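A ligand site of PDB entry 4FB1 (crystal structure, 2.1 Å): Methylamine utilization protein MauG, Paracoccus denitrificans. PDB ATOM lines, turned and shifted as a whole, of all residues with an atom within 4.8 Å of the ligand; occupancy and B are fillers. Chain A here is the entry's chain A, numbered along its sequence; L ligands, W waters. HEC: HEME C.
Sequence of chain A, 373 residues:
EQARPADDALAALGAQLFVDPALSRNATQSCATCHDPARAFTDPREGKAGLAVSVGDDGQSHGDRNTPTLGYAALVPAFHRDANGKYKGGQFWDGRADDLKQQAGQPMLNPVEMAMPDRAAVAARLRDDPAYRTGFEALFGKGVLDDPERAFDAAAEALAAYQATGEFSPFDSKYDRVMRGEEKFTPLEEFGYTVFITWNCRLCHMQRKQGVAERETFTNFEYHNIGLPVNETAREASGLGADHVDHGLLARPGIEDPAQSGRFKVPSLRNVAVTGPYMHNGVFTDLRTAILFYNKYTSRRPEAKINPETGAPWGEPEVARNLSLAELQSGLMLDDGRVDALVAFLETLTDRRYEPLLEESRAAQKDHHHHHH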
ATOM      1  N   PHE A  18      29.308 -19.046  23.600  1.00  0.00           N
ATOM      2  CA  PHE A  18      29.879 -18.373  22.453  1.00  0.00           C
ATOM      3  C   PHE A  18      30.332 -19.400  21.426  1.00  0.00           C
ATOM      4  O   PHE A  18      30.242 -19.157  20.200  1.00  0.00           O
ATOM      5  CB  PHE A  18      31.063 -17.540  22.892  1.00  0.00           C
ATOM      6  CG  PHE A  18      31.613 -16.668  21.807  1.00  0.00           C
ATOM      7  CD1 PHE A  18      31.144 -15.363  21.642  1.00  0.00           C
ATOM      8  CD2 PHE A  18      32.670 -17.102  21.022  1.00  0.00           C
ATOM      9  CE1 PHE A  18      31.670 -14.522  20.673  1.00  0.00           C
ATOM     10  CE2 PHE A  18      33.201 -16.262  20.006  1.00  0.00           C
ATOM     11  CZ  PHE A  18      32.701 -15.010  19.857  1.00  0.00           C
ATOM     12  N   GLN A  29      26.361 -24.308  14.000  1.00  0.00           N
ATOM     13  CA  GLN A  29      26.964 -22.985  13.963  1.00  0.00           C
ATOM     14  C   GLN A  29      26.919 -22.283  15.344  1.00  0.00           C
ATOM     15  O   GLN A  29      25.881 -22.267  16.005  1.00  0.00           O
ATOM     16  CB  GLN A  29      26.285 -22.135  12.872  1.00  0.00           C
ATOM     17  CG  GLN A  29      26.730 -20.695  12.783  1.00  0.00           C
ATOM     18  CD  GLN A  29      26.252 -19.977  11.510  1.00  0.00           C
ATOM     19  OE1 GLN A  29      26.756 -20.227  10.394  1.00  0.00           O
ATOM     20  NE2 GLN A  29      25.341 -19.026  11.684  1.00  0.00           N
ATOM     21  N   SER A  30      28.049 -21.738  15.790  1.00  0.00           N
ATOM     22  CA  SER A  30      28.018 -20.914  16.981  1.00  0.00           C
ATOM     23  C   SER A  30      28.553 -19.520  16.636  1.00  0.00           C
ATOM     24  O   SER A  30      28.935 -19.305  15.462  1.00  0.00           O
ATOM     25  CB  SER A  30      28.867 -21.580  18.055  1.00  0.00           C
ATOM     26  OG  SER A  30      30.203 -21.385  17.726  1.00  0.00           O
ATOM     27  N   CYS A  31      28.619 -18.606  17.624  1.00  0.00           N
ATOM     28  CA  CYS A  31      29.197 -17.258  17.364  1.00  0.00           C
ATOM     29  C   CYS A  31      30.633 -17.395  16.866  1.00  0.00           C
ATOM     30  O   CYS A  31      31.095 -16.641  15.998  1.00  0.00           O
ATOM     31  CB  CYS A  31      29.250 -16.374  18.600  1.00  0.00           C
ATOM     32  SG  CYS A  31      27.850 -16.408  19.734  1.00  0.00           S
ATOM     33  N   CYS A  34      31.596 -17.619  13.160  1.00  0.00           N
ATOM     34  CA  CYS A  34      31.798 -16.458  12.296  1.00  0.00           C
ATOM     35  C   CYS A  34      32.795 -15.510  12.909  1.00  0.00           C
ATOM     36  O   CYS A  34      33.486 -14.735  12.226  1.00  0.00           O
ATOM     37  CB  CYS A  34      30.501 -15.738  12.057  1.00  0.00           C
ATOM     38  SG  CYS A  34      29.414 -16.644  11.040  1.00  0.00           S
ATOM     39  N   HIS A  35      32.808 -15.519  14.226  1.00  0.00           N
ATOM     40  CA  HIS A  35      33.725 -14.670  14.929  1.00  0.00           C
ATOM     41  C   HIS A  35      34.772 -15.655  15.439  1.00  0.00           C
ATOM     42  O   HIS A  35      34.827 -15.978  16.623  1.00  0.00           O
ATOM     43  CB  HIS A  35      32.988 -13.943  16.017  1.00  0.00           C
ATOM     44  CG  HIS A  35      31.911 -13.019  15.510  1.00  0.00           C
ATOM     45  ND1 HIS A  35      32.186 -11.781  14.964  1.00  0.00           N
ATOM     46  CD2 HIS A  35      30.563 -13.143  15.477  1.00  0.00           C
ATOM     47  CE1 HIS A  35      31.054 -11.174  14.643  1.00  0.00           C
ATOM     48  NE2 HIS A  35      30.052 -11.974  14.953  1.00  0.00           N
ATOM     49  N   ARG A  45      35.938 -18.366   6.788  1.00  0.00           N
ATOM     50  CA  ARG A  45      35.393 -19.390   5.852  1.00  0.00           C
ATOM     51  C   ARG A  45      35.033 -18.798   4.501  1.00  0.00           C
ATOM     52  O   ARG A  45      34.388 -17.737   4.460  1.00  0.00           O
ATOM     53  CB  ARG A  45      34.190 -20.175   6.405  1.00  0.00           C
ATOM     54  CG  ARG A  45      34.424 -21.105   7.605  1.00  0.00           C
ATOM     55  CD  ARG A  45      33.046 -21.413   8.274  1.00  0.00           C
ATOM     56  NE  ARG A  45      32.260 -20.157   8.411  1.00  0.00           N
ATOM     57  CZ  ARG A  45      30.931 -20.088   8.319  1.00  0.00           C
ATOM     58  NH1 ARG A  45      30.206 -21.204   8.130  1.00  0.00           N
ATOM     59  NH2 ARG A  45      30.337 -18.909   8.435  1.00  0.00           N
ATOM     60  N   SER A  54      29.534 -13.875   5.305  1.00  0.00           N
ATOM     61  CA  SER A  54      29.531 -15.195   5.953  1.00  0.00           C
ATOM     62  C   SER A  54      28.278 -15.992   5.613  1.00  0.00           C
ATOM     63  O   SER A  54      27.222 -15.392   5.306  1.00  0.00           O
ATOM     64  CB  SER A  54      29.601 -15.019   7.474  1.00  0.00           C
ATOM     65  OG  SER A  54      30.726 -14.235   7.856  1.00  0.00           O
ATOM     66  N   VAL A  55      28.398 -17.325   5.725  1.00  0.00           N
ATOM     67  CA  VAL A  55      27.265 -18.229   5.540  1.00  0.00           C
ATOM     68  C   VAL A  55      26.553 -18.610   6.851  1.00  0.00           C
ATOM     69  O   VAL A  55      27.190 -18.941   7.862  1.00  0.00           O
ATOM     70  CB  VAL A  55      27.715 -19.465   4.759  1.00  0.00           C
ATOM     71  CG1 VAL A  55      26.608 -20.538   4.654  1.00  0.00           C
ATOM     72  CG2 VAL A  55      28.177 -19.007   3.396  1.00  0.00           C
ATOM     73  N   GLY A  56      25.216 -18.544   6.823  1.00  0.00           N
ATOM     74  CA  GLY A  56      24.415 -18.965   7.962  1.00  0.00           C
ATOM     75  C   GLY A  56      24.408 -20.475   8.246  1.00  0.00           C
ATOM     76  O   GLY A  56      25.027 -21.281   7.519  1.00  0.00           O
ATOM     77  N   ARG A  65      26.765  -7.991   4.782  1.00  0.00           N
ATOM     78  CA  ARG A  65      27.892  -7.316   5.362  1.00  0.00           C
ATOM     79  C   ARG A  65      29.018  -8.243   5.810  1.00  0.00           C
ATOM     80  O   ARG A  65      28.796  -9.422   6.119  1.00  0.00           O
ATOM     81  CB  ARG A  65      27.431  -6.423   6.507  1.00  0.00           C
ATOM     82  CG  ARG A  65      26.704  -5.194   6.002  1.00  0.00           C
ATOM     83  CD  ARG A  65      25.795  -4.732   7.076  1.00  0.00           C
ATOM     84  NE  ARG A  65      25.023  -3.544   6.682  1.00  0.00           N
ATOM     85  CZ  ARG A  65      24.282  -2.859   7.533  1.00  0.00           C
ATOM     86  NH1 ARG A  65      24.234  -3.224   8.826  1.00  0.00           N
ATOM     87  NH2 ARG A  65      23.610  -1.787   7.119  1.00  0.00           N
ATOM     88  N   ASN A  66      30.235  -7.704   5.793  1.00  0.00           N
ATOM     89  CA  ASN A  66      31.430  -8.354   6.363  1.00  0.00           C
ATOM     90  C   ASN A  66      31.306  -8.486   7.889  1.00  0.00           C
ATOM     91  O   ASN A  66      30.853  -7.535   8.655  1.00  0.00           O
ATOM     92  CB  ASN A  66      32.666  -7.542   5.953  1.00  0.00           C
ATOM     93  CG  ASN A  66      33.969  -8.182   6.319  1.00  0.00           C
ATOM     94  OD1 ASN A  66      34.760  -7.573   7.083  1.00  0.00           O
ATOM     95  ND2 ASN A  66      34.259  -9.429   5.764  1.00  0.00           N
ATOM     96  N   THR A  67      31.633  -9.693   8.331  1.00  0.00           N
ATOM     97  CA  THR A  67      31.581 -10.005   9.740  1.00  0.00           C
ATOM     98  C   THR A  67      32.764  -9.272  10.420  1.00  0.00           C
ATOM     99  O   THR A  67      33.946  -9.467  10.082  1.00  0.00           O
ATOM    100  CB  THR A  67      31.616 -11.531   9.932  1.00  0.00           C
ATOM    101  OG1 THR A  67      30.443 -12.111   9.368  1.00  0.00           O
ATOM    102  CG2 THR A  67      31.736 -11.894  11.418  1.00  0.00           C
ATOM    103  N   PRO A  68      32.437  -8.346  11.328  1.00  0.00           N
ATOM    104  CA  PRO A  68      33.483  -7.563  11.941  1.00  0.00           C
ATOM    105  C   PRO A  68      34.122  -8.305  13.153  1.00  0.00           C
ATOM    106  O   PRO A  68      33.554  -9.254  13.726  1.00  0.00           O
ATOM    107  CB  PRO A  68      32.742  -6.280  12.394  1.00  0.00           C
ATOM    108  CG  PRO A  68      31.379  -6.772  12.720  1.00  0.00           C
ATOM    109  CD  PRO A  68      31.100  -7.940  11.797  1.00  0.00           C
ATOM    110  N   THR A  69      35.296  -7.829  13.562  1.00  0.00           N
ATOM    111  CA  THR A  69      35.925  -8.342  14.760  1.00  0.00           C
ATOM    112  C   THR A  69      35.067  -8.038  15.971  1.00  0.00           C
ATOM    113  O   THR A  69      34.375  -7.026  15.976  1.00  0.00           O
ATOM    114  CB  THR A  69      37.255  -7.645  14.985  1.00  0.00           C
ATOM    115  OG1 THR A  69      37.891  -8.281  16.085  1.00  0.00           O
ATOM    116  CG2 THR A  69      37.030  -6.099  15.293  1.00  0.00           C
ATOM    117  N   LEU A  70      35.153  -8.863  17.000  1.00  0.00           N
ATOM    118  CA  LEU A  70      34.517  -8.505  18.296  1.00  0.00           C
ATOM    119  C   LEU A  70      35.534  -7.905  19.299  1.00  0.00           C
ATOM    120  O   LEU A  70      35.164  -7.478  20.391  1.00  0.00           O
ATOM    121  CB  LEU A  70      33.843  -9.735  18.896  1.00  0.00           C
ATOM    122  CG  LEU A  70      32.825 -10.457  18.013  1.00  0.00           C
ATOM    123  CD1 LEU A  70      32.143 -11.478  18.843  1.00  0.00           C
ATOM    124  CD2 LEU A  70      31.809  -9.458  17.426  1.00  0.00           C
ATOM    125  N   ALA A  73      35.193  -4.228  20.816  1.00  0.00           N
ATOM    126  CA  ALA A  73      33.795  -3.790  20.628  1.00  0.00           C
ATOM    127  C   ALA A  73      33.184  -3.372  21.967  1.00  0.00           C
ATOM    128  O   ALA A  73      32.289  -2.507  22.009  1.00  0.00           O
ATOM    129  CB  ALA A  73      32.950  -4.861  19.906  1.00  0.00           C
ATOM    130  N   GLN A  91      26.216  -0.849  17.957  1.00  0.00           N
ATOM    131  CA  GLN A  91      26.823  -2.086  17.477  1.00  0.00           C
ATOM    132  C   GLN A  91      26.217  -2.497  16.127  1.00  0.00           C
ATOM    133  O   GLN A  91      25.088  -2.156  15.836  1.00  0.00           O
ATOM    134  CB  GLN A  91      26.644  -3.218  18.509  1.00  0.00           C
ATOM    135  CG  GLN A  91      27.334  -2.952  19.820  1.00  0.00           C
ATOM    136  CD  GLN A  91      28.871  -2.983  19.761  1.00  0.00           C
ATOM    137  OE1 GLN A  91      29.562  -2.514  20.689  1.00  0.00           O
ATOM    138  NE2 GLN A  91      29.411  -3.586  18.741  1.00  0.00           N
ATOM    139  N   PHE A  92      26.996  -3.234  15.326  1.00  0.00           N
ATOM    140  CA  PHE A  92      26.728  -3.490  13.890  1.00  0.00           C
ATOM    141  C   PHE A  92      27.184  -2.261  13.104  1.00  0.00           C
ATOM    142  O   PHE A  92      27.266  -1.132  13.649  1.00  0.00           O
ATOM    143  CB  PHE A  92      25.239  -3.700  13.494  1.00  0.00           C
ATOM    144  CG  PHE A  92      24.604  -4.964  14.010  1.00  0.00           C
ATOM    145  CD1 PHE A  92      25.085  -6.207  13.638  1.00  0.00           C
ATOM    146  CD2 PHE A  92      23.461  -4.887  14.811  1.00  0.00           C
ATOM    147  CE1 PHE A  92      24.481  -7.384  14.114  1.00  0.00           C
ATOM    148  CE2 PHE A  92      22.836  -6.036  15.242  1.00  0.00           C
ATOM    149  CZ  PHE A  92      23.362  -7.294  14.902  1.00  0.00           C
ATOM    150  N   TRP A  93      27.347  -2.465  11.807  1.00  0.00           N
ATOM    151  CA  TRP A  93      27.962  -1.450  10.986  1.00  0.00           C
ATOM    152  C   TRP A  93      27.059  -0.228  10.806  1.00  0.00           C
ATOM    153  O   TRP A  93      27.511   0.803  10.292  1.00  0.00           O
ATOM    154  CB  TRP A  93      28.262  -2.014   9.619  1.00  0.00           C
ATOM    155  CG  TRP A  93      29.403  -2.912   9.507  1.00  0.00           C
ATOM    156  CD1 TRP A  93      29.355  -4.301   9.428  1.00  0.00           C
ATOM    157  CD2 TRP A  93      30.761  -2.542   9.277  1.00  0.00           C
ATOM    158  NE1 TRP A  93      30.621  -4.798   9.195  1.00  0.00           N
ATOM    159  CE2 TRP A  93      31.501  -3.743   9.098  1.00  0.00           C
ATOM    160  CE3 TRP A  93      31.430  -1.305   9.174  1.00  0.00           C
ATOM    161  CZ2 TRP A  93      32.888  -3.739   8.860  1.00  0.00           C
ATOM    162  CZ3 TRP A  93      32.812  -1.301   8.912  1.00  0.00           C
ATOM    163  CH2 TRP A  93      33.520  -2.504   8.764  1.00  0.00           C
ATOM    164  N   ASP A  94      25.781  -0.389  11.183  1.00  0.00           N
ATOM    165  CA  ASP A  94      24.805   0.670  11.007  1.00  0.00           C
ATOM    166  C   ASP A  94      24.251   1.034  12.349  1.00  0.00           C
ATOM    167  O   ASP A  94      23.208   1.651  12.448  1.00  0.00           O
ATOM    168  CB  ASP A  94      23.681   0.261  10.037  1.00  0.00           C
ATOM    169  CG  ASP A  94      22.981  -1.027  10.452  1.00  0.00           C
ATOM    170  OD1 ASP A  94      22.117  -1.489   9.687  1.00  0.00           O
ATOM    171  OD2 ASP A  94      23.302  -1.571  11.529  1.00  0.00           O
ATOM    172  N   ARG A  96      22.485  -0.311  14.490  1.00  0.00           N
ATOM    173  CA  ARG A  96      21.081  -0.560  14.771  1.00  0.00           C
ATOM    174  C   ARG A  96      20.850  -1.254  16.150  1.00  0.00           C
ATOM    175  O   ARG A  96      19.714  -1.350  16.626  1.00  0.00           O
ATOM    176  CB  ARG A  96      20.491  -1.384  13.621  1.00  0.00           C
ATOM    177  CG  ARG A  96      20.871  -2.907  13.667  1.00  0.00           C
ATOM    178  CD  ARG A  96      20.170  -3.660  12.504  1.00  0.00           C
ATOM    179  NE  ARG A  96      20.572  -5.056  12.350  1.00  0.00           N
ATOM    180  CZ  ARG A  96      21.687  -5.430  11.718  1.00  0.00           C
ATOM    181  NH1 ARG A  96      21.980  -6.713  11.594  1.00  0.00           N
ATOM    182  NH2 ARG A  96      22.516  -4.503  11.226  1.00  0.00           N
ATOM    183  N   LEU A 100      26.165  -4.122  23.375  1.00  0.00           N
ATOM    184  CA  LEU A 100      26.523  -5.520  23.150  1.00  0.00           C
ATOM    185  C   LEU A 100      25.384  -6.429  23.608  1.00  0.00           C
ATOM    186  O   LEU A 100      25.105  -7.439  22.977  1.00  0.00           O
ATOM    187  CB  LEU A 100      27.779  -5.885  23.877  1.00  0.00           C
ATOM    188  CG  LEU A 100      29.023  -5.447  23.143  1.00  0.00           C
ATOM    189  CD1 LEU A 100      30.189  -5.757  24.123  1.00  0.00           C
ATOM    190  CD2 LEU A 100      29.155  -6.114  21.726  1.00  0.00           C
ATOM    191  N   GLN A 103      22.654  -6.428  20.948  1.00  0.00           N
ATOM    192  CA  GLN A 103      23.174  -7.088  19.751  1.00  0.00           C
ATOM    193  C   GLN A 103      23.152  -8.648  19.894  1.00  0.00           C
ATOM    194  O   GLN A 103      22.693  -9.337  18.991  1.00  0.00           O
ATOM    195  CB  GLN A 103      24.577  -6.576  19.409  1.00  0.00           C
ATOM    196  CG  GLN A 103      25.100  -7.082  18.039  1.00  0.00           C
ATOM    197  CD  GLN A 103      25.330  -8.571  18.048  1.00  0.00           C
ATOM    198  OE1 GLN A 103      25.589  -9.156  19.111  1.00  0.00           O
ATOM    199  NE2 GLN A 103      25.234  -9.204  16.880  1.00  0.00           N
ATOM    200  N   ALA A 104      23.641  -9.188  21.022  1.00  0.00           N
ATOM    201  CA  ALA A 104      23.834 -10.648  21.227  1.00  0.00           C
ATOM    202  C   ALA A 104      22.758 -11.553  20.677  1.00  0.00           C
ATOM    203  O   ALA A 104      23.044 -12.527  19.963  1.00  0.00           O
ATOM    204  CB  ALA A 104      24.145 -10.990  22.763  1.00  0.00           C
ATOM    205  N   PRO A 107      21.856 -12.400  16.233  1.00  0.00           N
ATOM    206  CA  PRO A 107      22.345 -13.543  15.401  1.00  0.00           C
ATOM    207  C   PRO A 107      21.616 -14.900  15.582  1.00  0.00           C
ATOM    208  O   PRO A 107      21.406 -15.605  14.601  1.00  0.00           O
ATOM    209  CB  PRO A 107      23.817 -13.693  15.832  1.00  0.00           C
ATOM    210  CG  PRO A 107      24.192 -12.293  16.330  1.00  0.00           C
ATOM    211  CD  PRO A 107      22.940 -11.825  17.038  1.00  0.00           C
ATOM    212  N   MET A 108      21.283 -15.235  16.829  1.00  0.00           N
ATOM    213  CA  MET A 108      20.503 -16.437  17.155  1.00  0.00           C
ATOM    214  C   MET A 108      19.206 -16.585  16.416  1.00  0.00           C
ATOM    215  O   MET A 108      18.807 -17.716  16.104  1.00  0.00           O
ATOM    216  CB  MET A 108      20.153 -16.474  18.629  1.00  0.00           C
ATOM    217  CG  MET A 108      21.365 -16.372  19.503  1.00  0.00           C
ATOM    218  SD  MET A 108      20.989 -16.682  21.221  1.00  0.00           S
ATOM    219  CE  MET A 108      22.352 -15.700  21.884  1.00  0.00           C
ATOM    220  N   VAL A 112      19.220 -15.776   8.182  1.00  0.00           N
ATOM    221  CA  VAL A 112      20.424 -15.827   7.316  1.00  0.00           C
ATOM    222  C   VAL A 112      21.694 -16.101   8.173  1.00  0.00           C
ATOM    223  O   VAL A 112      22.792 -16.215   7.638  1.00  0.00           O
ATOM    224  CB  VAL A 112      20.592 -14.542   6.322  1.00  0.00           C
ATOM    225  CG1 VAL A 112      19.300 -13.690   6.225  1.00  0.00           C
ATOM    226  CG2 VAL A 112      21.720 -13.633   6.708  1.00  0.00           C
ATOM    227  N   GLU A 113      21.539 -16.175   9.499  1.00  0.00           N
ATOM    228  CA  GLU A 113      22.640 -16.563  10.380  1.00  0.00           C
ATOM    229  C   GLU A 113      22.327 -17.847  11.174  1.00  0.00           C
ATOM    230  O   GLU A 113      22.257 -18.960  10.598  1.00  0.00           O
ATOM    231  CB  GLU A 113      23.092 -15.397  11.295  1.00  0.00           C
ATOM    232  CG  GLU A 113      23.619 -14.197  10.477  1.00  0.00           C
ATOM    233  CD  GLU A 113      23.723 -12.860  11.309  1.00  0.00           C
ATOM    234  OE1 GLU A 113      23.016 -12.685  12.328  1.00  0.00           O
ATOM    235  OE2 GLU A 113      24.547 -11.995  10.923  1.00  0.00           O
ATOM    236  N   MET A 114      22.130 -17.721  12.482  1.00  0.00           N
ATOM    237  CA  MET A 114      21.962 -18.916  13.309  1.00  0.00           C
ATOM    238  C   MET A 114      20.574 -19.537  13.202  1.00  0.00           C
ATOM    239  O   MET A 114      20.399 -20.733  13.444  1.00  0.00           O
ATOM    240  CB  MET A 114      22.397 -18.644  14.750  1.00  0.00           C
ATOM    241  CG  MET A 114      23.852 -18.184  14.825  1.00  0.00           C
ATOM    242  SD  MET A 114      24.430 -17.666  16.469  1.00  0.00           S
ATOM    243  CE  MET A 114      24.884 -19.309  17.057  1.00  0.00           C
ATOM    244  N   LEU A 159      26.722 -13.444  26.964  1.00  0.00           N
ATOM    245  CA  LEU A 159      27.556 -13.133  25.768  1.00  0.00           C
ATOM    246  C   LEU A 159      28.264 -11.762  25.900  1.00  0.00           C
ATOM    247  O   LEU A 159      29.481 -11.665  25.629  1.00  0.00           O
ATOM    248  CB  LEU A 159      26.751 -13.281  24.475  1.00  0.00           C
ATOM    249  CG  LEU A 159      26.572 -14.811  24.209  1.00  0.00           C
ATOM    250  CD1 LEU A 159      25.328 -15.104  23.320  1.00  0.00           C
ATOM    251  CD2 LEU A 159      27.851 -15.510  23.640  1.00  0.00           C
ATOM    252  N   GLN A 163      32.189 -10.819  26.049  1.00  0.00           N
ATOM    253  CA  GLN A 163      32.916  -9.906  25.123  1.00  0.00           C
ATOM    254  C   GLN A 163      33.538  -8.703  25.822  1.00  0.00           C
ATOM    255  O   GLN A 163      34.258  -7.963  25.149  1.00  0.00           O
ATOM    256  CB  GLN A 163      32.029  -9.401  23.975  1.00  0.00           C
ATOM    257  CG  GLN A 163      31.537 -10.491  23.063  1.00  0.00           C
ATOM    258  CD  GLN A 163      30.383 -10.066  22.193  1.00  0.00           C
ATOM    259  OE1 GLN A 163      29.223 -10.240  22.588  1.00  0.00           O
ATOM    260  NE2 GLN A 163      30.671  -9.489  21.019  1.00  0.00           N
ATOM    261  N   LYS A 265      29.378   2.880  10.796  1.00  0.00           N
ATOM    262  CA  LYS A 265      30.152   3.164  12.008  1.00  0.00           C
ATOM    263  C   LYS A 265      31.635   3.079  11.691  1.00  0.00           C
ATOM    264  O   LYS A 265      32.055   2.132  11.039  1.00  0.00           O
ATOM    265  CB  LYS A 265      29.780   2.127  13.098  1.00  0.00           C
ATOM    266  CG  LYS A 265      30.700   2.077  14.323  1.00  0.00           C
ATOM    267  CD  LYS A 265      29.984   1.302  15.482  1.00  0.00           C
ATOM    268  CE  LYS A 265      29.846  -0.250  15.281  1.00  0.00           C
ATOM    269  NZ  LYS A 265      31.089  -1.064  14.907  1.00  0.00           N
HETATM  270 FE   HEC L   1      28.028 -11.508  14.817  1.00  0.00          FE
HETATM  271  CHA HEC L   1      28.274  -8.217  13.965  1.00  0.00           C
HETATM  272  CHB HEC L   1      28.402 -10.684  18.106  1.00  0.00           C
HETATM  273  CHC HEC L   1      26.986 -14.727  15.702  1.00  0.00           C
HETATM  274  CHD HEC L   1      28.308 -12.454  11.645  1.00  0.00           C
HETATM  275  NA  HEC L   1      28.304  -9.721  15.848  1.00  0.00           N
HETATM  276  C1A HEC L   1      28.369  -8.497  15.380  1.00  0.00           C
HETATM  277  C2A HEC L   1      28.578  -7.452  16.421  1.00  0.00           C
HETATM  278  C3A HEC L   1      28.567  -8.144  17.603  1.00  0.00           C
HETATM  279  C4A HEC L   1      28.385  -9.547  17.176  1.00  0.00           C
HETATM  280  CMA HEC L   1      28.746  -7.586  18.980  1.00  0.00           C
HETATM  281  CAA HEC L   1      28.742  -5.975  16.251  1.00  0.00           C
HETATM  282  CBA HEC L   1      30.243  -5.773  15.933  1.00  0.00           C
HETATM  283  CGA HEC L   1      30.547  -4.291  15.586  1.00  0.00           C
HETATM  284  O1A HEC L   1      31.724  -3.845  15.619  1.00  0.00           O
HETATM  285  O2A HEC L   1      29.639  -3.523  15.243  1.00  0.00           O
HETATM  286  NB  HEC L   1      27.754 -12.528  16.612  1.00  0.00           N
HETATM  287  C1B HEC L   1      27.930 -12.052  17.832  1.00  0.00           C
HETATM  288  C2B HEC L   1      27.577 -13.003  18.921  1.00  0.00           C
HETATM  289  C3B HEC L   1      27.157 -14.130  18.248  1.00  0.00           C
HETATM  290  C4B HEC L   1      27.294 -13.788  16.819  1.00  0.00           C
HETATM  291  CMB HEC L   1      27.656 -12.734  20.407  1.00  0.00           C
HETATM  292  CAB HEC L   1      26.670 -15.398  18.863  1.00  0.00           C
HETATM  293  CBB HEC L   1      25.209 -15.204  19.185  1.00  0.00           C
HETATM  294  NC  HEC L   1      27.687 -13.293  13.789  1.00  0.00           N
HETATM  295  C1C HEC L   1      27.369 -14.513  14.287  1.00  0.00           C
HETATM  296  C2C HEC L   1      27.388 -15.605  13.283  1.00  0.00           C
HETATM  297  C3C HEC L   1      27.767 -14.988  12.109  1.00  0.00           C
HETATM  298  C4C HEC L   1      27.928 -13.545  12.517  1.00  0.00           C
HETATM  299  CMC HEC L   1      27.082 -17.060  13.539  1.00  0.00           C
HETATM  300  CAC HEC L   1      27.974 -15.605  10.733  1.00  0.00           C
HETATM  301  CBC HEC L   1      26.694 -16.171  10.182  1.00  0.00           C
HETATM  302  ND  HEC L   1      28.314 -10.494  13.040  1.00  0.00           N
HETATM  303  C1D HEC L   1      28.168 -10.998  11.841  1.00  0.00           C
HETATM  304  C2D HEC L   1      27.951  -9.993  10.787  1.00  0.00           C
HETATM  305  C3D HEC L   1      27.917  -8.776  11.474  1.00  0.00           C
HETATM  306  C4D HEC L   1      28.148  -9.181  12.866  1.00  0.00           C
HETATM  307  CMD HEC L   1      27.707 -10.197   9.328  1.00  0.00           C
HETATM  308  CAD HEC L   1      27.693  -7.379  10.977  1.00  0.00           C
HETATM  309  CBD HEC L   1      26.285  -7.379  10.415  1.00  0.00           C
HETATM  310  CGD HEC L   1      25.730  -5.978  10.374  1.00  0.00           C
HETATM  311  O1D HEC L   1      24.489  -5.894  10.208  1.00  0.00           O
HETATM  312  O2D HEC L   1      26.491  -4.982  10.465  1.00  0.00           O
HETATM  313  O   HOH W   1      24.976 -10.508  13.421  1.00  0.00           O
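NH2 of Arg 96 lies within salt-bridge range of OD2 of Asp 94, 3.1 Å away.
The backbone NH (N) of Lys 265 sits at hydrogen-bond distance from the backbone carbonyl oxygen (O) of Trp 93 (2.8 Å).
The indole nitrogen of Trp 93 is in hydrogen-bond range of the backbone carbonyl oxygen of Asn 66.
The side-chain carboxylate of Asp 94 is in salt-bridge range of the guanidinium group of Arg 65 (2.9 Å).
OG1 of Thr 67 is in hydrogen-bond range of OG of Ser 54, 2.6 Å away.
OE1 of Gln 29 lies close to O of Val 55, 2.9 Å away.
OE1 of Gln 91 lies close to O of Ala 73 (3.0 Å).
The backbone carbonyl oxygen (O) of Phe 18 lies within hydrogen-bond range of the side-chain hydroxyl (OG) of Ser 30 (3.3 Å).
NE2 of Gln 103 lies close to NA of the ligand, 3.3 Å away.
Gln 29 touches the ligand (NE2 to CMC, 3.2 Å).
Ser 30 touches the ligand.
CB of Ser 54 touches CAC of the ligand (3.7 Å).
O of Val 55 touches CBC of the ligand (3.6 Å).
Asn 66 touches the ligand (O to CAD, 3.9 Å).
OG1 of Thr 67 touches CHD of the ligand, at 3.1 Å.
Pro 68 touches the ligand.
Leu 70 touches the ligand (CD2 to C4A, 3.4 Å).
NE2 of Gln 91 touches CGA of the ligand (3.4 Å).
CD2 of Leu 100 touches CMA of the ligand, 3.1 Å away.
O of Ala 104 touches CBB of the ligand (3.5 Å).
Pro 107 touches the ligand (CB to CHC, 3.3 Å).
CE of Met 108 touches CBB of the ligand (3.96 Å).
CG of Glu 113 touches CBC of the ligand, 3.7 Å away.
CG of Met 114 touches CMC of the ligand, 3.7 Å away.
NE2 of Gln 163 touches CMA of the ligand, 3.4 Å away.
SG of Cys 31 is bonded to CAB of the ligand (1.8 Å).
A carbon (CAC) of the ligand is bonded to the side-chain sulfur of Cys 34 (1.8 Å).
An iron atom (FE) of the ligand is bound by a ring nitrogen (NE2) of His 35 (2.1 Å).
An oxygen (O1D) of the ligand is in salt-bridge range of the guanidinium group (NH2) of Arg 96, 2.6 Å away.
N of Phe 92 sits at hydrogen-bond distance from O2A of the ligand (2.7 Å).
O2A of the ligand lies within salt-bridge range of NZ of Lys 265 (2.9 Å).
The backbone NH of Trp 93 lies within hydrogen-bond range of an oxygen (O2D) of the ligand (3.0 Å).
O1D of the ligand lies within salt-bridge range of NH1 of Arg 65 (3.0 Å).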
